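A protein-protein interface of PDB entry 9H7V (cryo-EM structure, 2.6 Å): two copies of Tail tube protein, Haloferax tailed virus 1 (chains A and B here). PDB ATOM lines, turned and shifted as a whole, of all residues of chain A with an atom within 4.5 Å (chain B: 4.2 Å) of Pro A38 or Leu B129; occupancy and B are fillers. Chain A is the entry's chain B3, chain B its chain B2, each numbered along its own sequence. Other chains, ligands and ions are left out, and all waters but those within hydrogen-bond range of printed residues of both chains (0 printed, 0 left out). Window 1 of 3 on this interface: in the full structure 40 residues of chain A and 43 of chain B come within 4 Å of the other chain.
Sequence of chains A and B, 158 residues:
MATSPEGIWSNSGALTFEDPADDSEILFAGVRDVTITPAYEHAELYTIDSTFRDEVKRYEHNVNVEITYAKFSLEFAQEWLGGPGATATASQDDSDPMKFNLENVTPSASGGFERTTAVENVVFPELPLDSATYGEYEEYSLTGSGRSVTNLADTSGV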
ATOM      1  N   ILE A  36     -25.250 -12.076  15.718  1.00  0.00           N
ATOM      2  CA  ILE A  36     -25.731 -13.433  15.497  1.00  0.00           C
ATOM      3  C   ILE A  36     -27.122 -13.547  16.119  1.00  0.00           C
ATOM      4  O   ILE A  36     -27.288 -13.334  17.319  1.00  0.00           O
ATOM      5  CB  ILE A  36     -24.748 -14.493  16.043  1.00  0.00           C
ATOM      6  CG1 ILE A  36     -23.366 -14.401  15.390  1.00  0.00           C
ATOM      7  CG2 ILE A  36     -25.334 -15.894  15.914  1.00  0.00           C
ATOM      8  CD1 ILE A  36     -22.242 -14.984  16.222  1.00  0.00           C
ATOM      9  N   THR A  37     -28.110 -13.885  15.280  1.00  0.00           N
ATOM     10  CA  THR A  37     -29.504 -13.975  15.684  1.00  0.00           C
ATOM     11  C   THR A  37     -30.124 -15.243  15.095  1.00  0.00           C
ATOM     12  O   THR A  37     -30.391 -15.288  13.895  1.00  0.00           O
ATOM     13  CB  THR A  37     -30.283 -12.727  15.239  1.00  0.00           C
ATOM     14  OG1 THR A  37     -29.661 -11.567  15.790  1.00  0.00           O
ATOM     15  CG2 THR A  37     -31.743 -12.748  15.637  1.00  0.00           C
ATOM     16  N   PRO A  38     -30.346 -16.319  15.890  1.00  0.00           N
ATOM     17  CA  PRO A  38     -31.295 -17.365  15.511  1.00  0.00           C
ATOM     18  C   PRO A  38     -32.715 -16.809  15.448  1.00  0.00           C
ATOM     19  O   PRO A  38     -33.149 -16.090  16.347  1.00  0.00           O
ATOM     20  CB  PRO A  38     -31.165 -18.423  16.618  1.00  0.00           C
ATOM     21  CG  PRO A  38     -30.548 -17.677  17.778  1.00  0.00           C
ATOM     22  CD  PRO A  38     -29.643 -16.643  17.141  1.00  0.00           C
ATOM     23  N   ALA A  39     -33.413 -17.148  14.359  1.00  0.00           N
ATOM     24  CA  ALA A  39     -34.750 -16.651  14.085  1.00  0.00           C
ATOM     25  C   ALA A  39     -35.626 -17.783  13.560  1.00  0.00           C
ATOM     26  O   ALA A  39     -35.155 -18.658  12.838  1.00  0.00           O
ATOM     27  CB  ALA A  39     -34.674 -15.521  13.088  1.00  0.00           C
ATOM     28  N   HIS A  61     -36.521 -21.905  10.092  1.00  0.00           N
ATOM     29  CA  HIS A  61     -35.436 -21.472  10.957  1.00  0.00           C
ATOM     30  C   HIS A  61     -34.240 -21.030  10.119  1.00  0.00           C
ATOM     31  O   HIS A  61     -33.905 -21.676   9.128  1.00  0.00           O
ATOM     32  CB  HIS A  61     -35.054 -22.611  11.914  1.00  0.00           C
ATOM     33  CG  HIS A  61     -33.990 -22.263  12.900  1.00  0.00           C
ATOM     34  ND1 HIS A  61     -34.160 -21.277  13.851  1.00  0.00           N
ATOM     35  CD2 HIS A  61     -32.758 -22.775  13.103  1.00  0.00           C
ATOM     36  CE1 HIS A  61     -33.075 -21.190  14.590  1.00  0.00           C
ATOM     37  NE2 HIS A  61     -32.199 -22.095  14.148  1.00  0.00           N
ATOM     38  N   ASN A  62     -33.613 -19.921  10.537  1.00  0.00           N
ATOM     39  CA  ASN A  62     -32.299 -19.519  10.057  1.00  0.00           C
ATOM     40  C   ASN A  62     -31.573 -18.747  11.158  1.00  0.00           C
ATOM     41  O   ASN A  62     -32.204 -18.241  12.086  1.00  0.00           O
ATOM     42  CB  ASN A  62     -32.350 -18.770   8.717  1.00  0.00           C
ATOM     43  CG  ASN A  62     -32.855 -17.343   8.799  1.00  0.00           C
ATOM     44  OD1 ASN A  62     -33.678 -17.008   9.649  1.00  0.00           O
ATOM     45  ND2 ASN A  62     -32.384 -16.494   7.900  1.00  0.00           N
ATOM     46  N   VAL A  63     -30.243 -18.681  11.039  1.00  0.00           N
ATOM     47  CA  VAL A  63     -29.430 -17.834  11.894  1.00  0.00           C
ATOM     48  C   VAL A  63     -28.916 -16.674  11.047  1.00  0.00           C
ATOM     49  O   VAL A  63     -28.131 -16.880  10.124  1.00  0.00           O
ATOM     50  CB  VAL A  63     -28.279 -18.611  12.568  1.00  0.00           C
ATOM     51  CG1 VAL A  63     -27.458 -17.721  13.488  1.00  0.00           C
ATOM     52  CG2 VAL A  63     -28.780 -19.827  13.329  1.00  0.00           C
ATOM     53  N   ARG A 115     -19.118 -17.171  26.986  1.00  0.00           N
ATOM     54  CA  ARG A 115     -20.169 -17.433  26.016  1.00  0.00           C
ATOM     55  C   ARG A 115     -19.538 -17.944  24.721  1.00  0.00           C
ATOM     56  O   ARG A 115     -18.840 -17.196  24.040  1.00  0.00           O
ATOM     57  CB  ARG A 115     -20.939 -16.129  25.784  1.00  0.00           C
ATOM     58  CG  ARG A 115     -22.397 -16.296  25.381  1.00  0.00           C
ATOM     59  CD  ARG A 115     -22.719 -16.019  23.922  1.00  0.00           C
ATOM     60  NE  ARG A 115     -22.222 -14.765  23.358  1.00  0.00           N
ATOM     61  CZ  ARG A 115     -22.723 -13.551  23.582  1.00  0.00           C
ATOM     62  NH1 ARG A 115     -22.178 -12.498  22.995  1.00  0.00           N
ATOM     63  NH2 ARG A 115     -23.761 -13.384  24.383  1.00  0.00           N
ATOM     64  N   THR A 117     -20.750 -19.231  21.114  1.00  0.00           N
ATOM     65  CA  THR A 117     -21.803 -19.403  20.127  1.00  0.00           C
ATOM     66  C   THR A 117     -21.208 -20.067  18.891  1.00  0.00           C
ATOM     67  O   THR A 117     -20.270 -19.541  18.295  1.00  0.00           O
ATOM     68  CB  THR A 117     -22.445 -18.067  19.726  1.00  0.00           C
ATOM     69  OG1 THR A 117     -22.745 -17.321  20.904  1.00  0.00           O
ATOM     70  CG2 THR A 117     -23.707 -18.234  18.906  1.00  0.00           C
ATOM     71  N   VAL A 149     -27.865 -23.010  15.259  1.00  0.00           N
ATOM     72  CA  VAL A 149     -26.912 -22.845  16.345  1.00  0.00           C
ATOM     73  C   VAL A 149     -26.563 -24.244  16.851  1.00  0.00           C
ATOM     74  O   VAL A 149     -27.454 -24.986  17.259  1.00  0.00           O
ATOM     75  CB  VAL A 149     -27.485 -21.953  17.468  1.00  0.00           C
ATOM     76  CG1 VAL A 149     -26.530 -21.815  18.644  1.00  0.00           C
ATOM     77  CG2 VAL A 149     -27.896 -20.578  16.961  1.00  0.00           C
ATOM     78  N   LEU A 152     -24.477 -23.240  22.332  1.00  0.00           N
ATOM     79  CA  LEU A 152     -24.551 -22.052  23.165  1.00  0.00           C
ATOM     80  C   LEU A 152     -24.402 -22.487  24.620  1.00  0.00           C
ATOM     81  O   LEU A 152     -25.314 -23.087  25.189  1.00  0.00           O
ATOM     82  CB  LEU A 152     -25.880 -21.326  22.923  1.00  0.00           C
ATOM     83  CG  LEU A 152     -26.120 -20.084  23.783  1.00  0.00           C
ATOM     84  CD1 LEU A 152     -25.270 -18.909  23.319  1.00  0.00           C
ATOM     85  CD2 LEU A 152     -27.588 -19.707  23.776  1.00  0.00           C
ATOM     86  N   PHE B  72     -26.462 -10.418  29.399  1.00  0.00           N
ATOM     87  CA  PHE B  72     -26.783 -11.665  28.722  1.00  0.00           C
ATOM     88  C   PHE B  72     -27.144 -12.748  29.734  1.00  0.00           C
ATOM     89  O   PHE B  72     -26.423 -12.955  30.708  1.00  0.00           O
ATOM     90  CB  PHE B  72     -25.633 -12.111  27.818  1.00  0.00           C
ATOM     91  CG  PHE B  72     -25.964 -13.282  26.930  1.00  0.00           C
ATOM     92  CD1 PHE B  72     -26.762 -13.108  25.806  1.00  0.00           C
ATOM     93  CD2 PHE B  72     -25.495 -14.557  27.217  1.00  0.00           C
ATOM     94  CE1 PHE B  72     -27.079 -14.181  24.985  1.00  0.00           C
ATOM     95  CE2 PHE B  72     -25.814 -15.630  26.396  1.00  0.00           C
ATOM     96  CZ  PHE B  72     -26.603 -15.441  25.281  1.00  0.00           C
ATOM     97  N   ALA B  77     -31.707 -17.626  27.161  1.00  0.00           N
ATOM     98  CA  ALA B  77     -31.336 -17.989  25.803  1.00  0.00           C
ATOM     99  C   ALA B  77     -31.547 -19.483  25.558  1.00  0.00           C
ATOM    100  O   ALA B  77     -32.045 -19.865  24.501  1.00  0.00           O
ATOM    101  CB  ALA B  77     -29.916 -17.563  25.525  1.00  0.00           C
ATOM    102  N   TRP B  80     -35.235 -20.365  25.449  1.00  0.00           N
ATOM    103  CA  TRP B  80     -35.776 -19.975  24.154  1.00  0.00           C
ATOM    104  C   TRP B  80     -35.471 -21.048  23.112  1.00  0.00           C
ATOM    105  O   TRP B  80     -36.339 -21.382  22.307  1.00  0.00           O
ATOM    106  CB  TRP B  80     -35.258 -18.593  23.726  1.00  0.00           C
ATOM    107  CG  TRP B  80     -35.817 -18.075  22.434  1.00  0.00           C
ATOM    108  CD1 TRP B  80     -36.901 -17.261  22.276  1.00  0.00           C
ATOM    109  CD2 TRP B  80     -35.305 -18.312  21.108  1.00  0.00           C
ATOM    110  NE1 TRP B  80     -37.102 -16.984  20.951  1.00  0.00           N
ATOM    111  CE2 TRP B  80     -36.141 -17.615  20.208  1.00  0.00           C
ATOM    112  CE3 TRP B  80     -34.230 -19.050  20.591  1.00  0.00           C
ATOM    113  CZ2 TRP B  80     -35.933 -17.634  18.828  1.00  0.00           C
ATOM    114  CZ3 TRP B  80     -34.023 -19.066  19.228  1.00  0.00           C
ATOM    115  CH2 TRP B  80     -34.865 -18.368  18.359  1.00  0.00           C
ATOM    116  N   GLU B 126     -37.328 -14.165  17.266  1.00  0.00           N
ATOM    117  CA  GLU B 126     -35.881 -14.209  17.131  1.00  0.00           C
ATOM    118  C   GLU B 126     -35.199 -13.818  18.439  1.00  0.00           C
ATOM    119  O   GLU B 126     -35.733 -13.033  19.221  1.00  0.00           O
ATOM    120  CB  GLU B 126     -35.412 -13.363  15.945  1.00  0.00           C
ATOM    121  CG  GLU B 126     -35.762 -11.889  16.041  1.00  0.00           C
ATOM    122  CD  GLU B 126     -35.601 -11.122  14.738  1.00  0.00           C
ATOM    123  OE1 GLU B 126     -36.226 -11.523  13.733  1.00  0.00           O
ATOM    124  OE2 GLU B 126     -34.850 -10.127  14.729  1.00  0.00           O
ATOM    125  N   LEU B 127     -34.003 -14.381  18.640  1.00  0.00           N
ATOM    126  CA  LEU B 127     -33.202 -14.159  19.830  1.00  0.00           C
ATOM    127  C   LEU B 127     -31.824 -13.657  19.406  1.00  0.00           C
ATOM    128  O   LEU B 127     -31.104 -14.366  18.706  1.00  0.00           O
ATOM    129  CB  LEU B 127     -33.114 -15.480  20.604  1.00  0.00           C
ATOM    130  CG  LEU B 127     -32.182 -15.508  21.816  1.00  0.00           C
ATOM    131  CD1 LEU B 127     -32.782 -14.749  22.991  1.00  0.00           C
ATOM    132  CD2 LEU B 127     -31.882 -16.940  22.220  1.00  0.00           C
ATOM    133  N   PRO B 128     -31.419 -12.420  19.785  1.00  0.00           N
ATOM    134  CA  PRO B 128     -30.043 -11.970  19.569  1.00  0.00           C
ATOM    135  C   PRO B 128     -29.104 -12.654  20.561  1.00  0.00           C
ATOM    136  O   PRO B 128     -29.280 -12.536  21.774  1.00  0.00           O
ATOM    137  CB  PRO B 128     -30.118 -10.448  19.771  1.00  0.00           C
ATOM    138  CG  PRO B 128     -31.306 -10.239  20.691  1.00  0.00           C
ATOM    139  CD  PRO B 128     -32.259 -11.383  20.409  1.00  0.00           C
ATOM    140  N   LEU B 129     -28.128 -13.395  20.022  1.00  0.00           N
ATOM    141  CA  LEU B 129     -27.170 -14.138  20.826  1.00  0.00           C
ATOM    142  C   LEU B 129     -25.884 -13.331  20.986  1.00  0.00           C
ATOM    143  O   LEU B 129     -25.400 -13.165  22.103  1.00  0.00           O
ATOM    144  CB  LEU B 129     -26.903 -15.508  20.192  1.00  0.00           C
ATOM    145  CG  LEU B 129     -27.960 -16.584  20.438  1.00  0.00           C
ATOM    146  CD1 LEU B 129     -27.491 -17.923  19.892  1.00  0.00           C
ATOM    147  CD2 LEU B 129     -28.283 -16.712  21.919  1.00  0.00           C
ATOM    148  N   ASP B 130     -25.343 -12.845  19.862  1.00  0.00           N
ATOM    149  CA  ASP B 130     -24.203 -11.943  19.860  1.00  0.00           C
ATOM    150  C   ASP B 130     -24.619 -10.639  19.189  1.00  0.00           C
ATOM    151  O   ASP B 130     -25.278 -10.660  18.152  1.00  0.00           O
ATOM    152  CB  ASP B 130     -22.978 -12.578  19.196  1.00  0.00           C
ATOM    153  CG  ASP B 130     -22.510 -13.845  19.893  1.00  0.00           C
ATOM    154  OD1 ASP B 130     -23.194 -14.875  19.754  1.00  0.00           O
ATOM    155  OD2 ASP B 130     -21.475 -13.782  20.585  1.00  0.00           O
ATOM    156  N   GLU B 138     -22.522  -5.214  24.629  1.00  0.00           N
ATOM    157  CA  GLU B 138     -23.476  -5.866  23.746  1.00  0.00           C
ATOM    158  C   GLU B 138     -24.896  -5.507  24.177  1.00  0.00           C
ATOM    159  O   GLU B 138     -25.258  -5.677  25.341  1.00  0.00           O
ATOM    160  CB  GLU B 138     -23.255  -7.379  23.725  1.00  0.00           C
ATOM    161  CG  GLU B 138     -21.937  -7.791  23.091  1.00  0.00           C
ATOM    162  CD  GLU B 138     -21.859  -9.215  22.563  1.00  0.00           C
ATOM    163  OE1 GLU B 138     -22.921  -9.840  22.363  1.00  0.00           O
ATOM    164  OE2 GLU B 138     -20.731  -9.693  22.341  1.00  0.00           O
ATOM    165  N   TYR B 140     -28.948  -6.045  23.330  1.00  0.00           N
ATOM    166  CA  TYR B 140     -29.808  -7.080  22.783  1.00  0.00           C
ATOM    167  C   TYR B 140     -31.247  -6.572  22.716  1.00  0.00           C
ATOM    168  O   TYR B 140     -31.759  -6.046  23.702  1.00  0.00           O
ATOM    169  CB  TYR B 140     -29.704  -8.337  23.654  1.00  0.00           C
ATOM    170  CG  TYR B 140     -28.308  -8.867  23.873  1.00  0.00           C
ATOM    171  CD1 TYR B 140     -27.646  -9.552  22.864  1.00  0.00           C
ATOM    172  CD2 TYR B 140     -27.652  -8.710  25.088  1.00  0.00           C
ATOM    173  CE1 TYR B 140     -26.365 -10.052  23.046  1.00  0.00           C
ATOM    174  CE2 TYR B 140     -26.373  -9.206  25.288  1.00  0.00           C
ATOM    175  CZ  TYR B 140     -25.728  -9.881  24.264  1.00  0.00           C
ATOM    176  OH  TYR B 140     -24.471 -10.376  24.453  1.00  0.00           O
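N of Leu B127 lies within hydrogen-bond range of O of Pro A38, at 3.0 Å. The backbone carbonyl oxygen of Ile A36 is in hydrogen-bond range of the backbone NH of Leu B129, 2.8 Å away. The backbone carbonyl oxygen (O) of Leu B129 is in hydrogen-bond range of the guanidinium group (NH2) of Arg A115 (2.8 Å). O of Asp B130 sits at hydrogen-bond distance from N of Ile A36 (2.8 Å). The guanidinium group (NH1) of Arg A115 lies within salt-bridge range of the side-chain carboxylate (OD2) of Asp B130, at 2.8 Å. The side-chain hydroxyl (OG1) of Thr A117 is in hydrogen-bond range of the side-chain carboxylate (OD1) of Asp B130 (2.7 Å). OE1 of Glu B138 is in salt-bridge range of NH1 of Arg A115 (2.8 Å). OH of Tyr B140 is in hydrogen-bond range of NH2 of Arg A115, at 3.1 Å.
The side-chain carboxylate of Glu B138 sits at hydrogen-bond distance from the side-chain hydroxyl of Tyr B140. O of Ala A39 is in hydrogen-bond range of ND1 of His A61, 3.0 Å away. N of Ala A39 is in hydrogen-bond range of O of Asn A62 (2.8 Å).
Printed residues of chain B within 4 Å of Pro A38: Trp B80, Glu B126, Leu B127 and Leu B129. His A61 touches none of the printed residues of chain B. Of the printed residues of chain B, Thr A117 touches Leu B129 (3.9 Å) and Asp B130 (2.7 Å). Of the printed residues of chain A, Glu B126 touches Thr A37 (3.7 Å), Pro A38 (3.4 Å) and Ala A39 (3.7 Å). Printed residues of chain A within 4 Å of Leu B127: Thr A37 and Pro A38. Leu B129 touches just these residues of chain A: Ile A36, Pro A38, Arg A115, Thr A117, Val A149 and Leu A152. The nearest printed residue of chain B that does not touch Pro A38 is Pro B128 (5.3 Å). The nearest printed residue of chain A that does not touch Glu B138 is Ile A36 (7.4 Å).
No position is printed for both chains. Of the 21 pairs that touch across the chains among the printed residues, none has its exchanged pair printed and touching as well.
Hydrophobic or aromatic side chains of chain A within 4 Å of the printed part of chain B: Ile A36, Pro A38, Ala A39, Val A149 and Leu A152. Of the 10 printed residues of chain B, 10 touch a printed residue of chain A. Printed residues of chain B that touch a printed residue of chain A: Phe B72, Ala B77, Trp B80, Glu B126, Leu B127, Pro B128, Leu B129, Asp B130, Glu B138 and Tyr B140. Hydrophobic or aromatic side chains of chain B that line the printed part of chain A: Phe B72, Ala B77, Trp B80, Leu B129 and Tyr B140. Among the printed residues, 21 pairs touch across the chains. Among the printed residues, Asp or Glu carboxylates within 4 Å of a Lys or Arg side-chain nitrogen of the other chain: Arg A115 with Asp B130 (2.8 Å) and Arg A115 with Glu B138 (2.8 Å).
O of Ile A36 touches C of Pro B128, 3.8 Å away. Thr A37 touches Glu B126. O of Leu B127 touches CA of Thr A37, 3.4 Å away. OG1 of Thr A37 touches CA of Pro B128 (3.8 Å). Pro A38 touches Trp B80 (O to CH2, 3.5 Å). Pro A38 touches Glu B126 (O to CA, 3.4 Å). Arg A115 touches Phe B72 (NH2 to CD1, 3.3 Å). CG2 of Thr A117 touches CD1 of Leu B129, at 3.9 Å. CD1 of Leu B129 touches CG2 of Val A149, at 3.98 Å. Leu A152 touches Ala B77.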
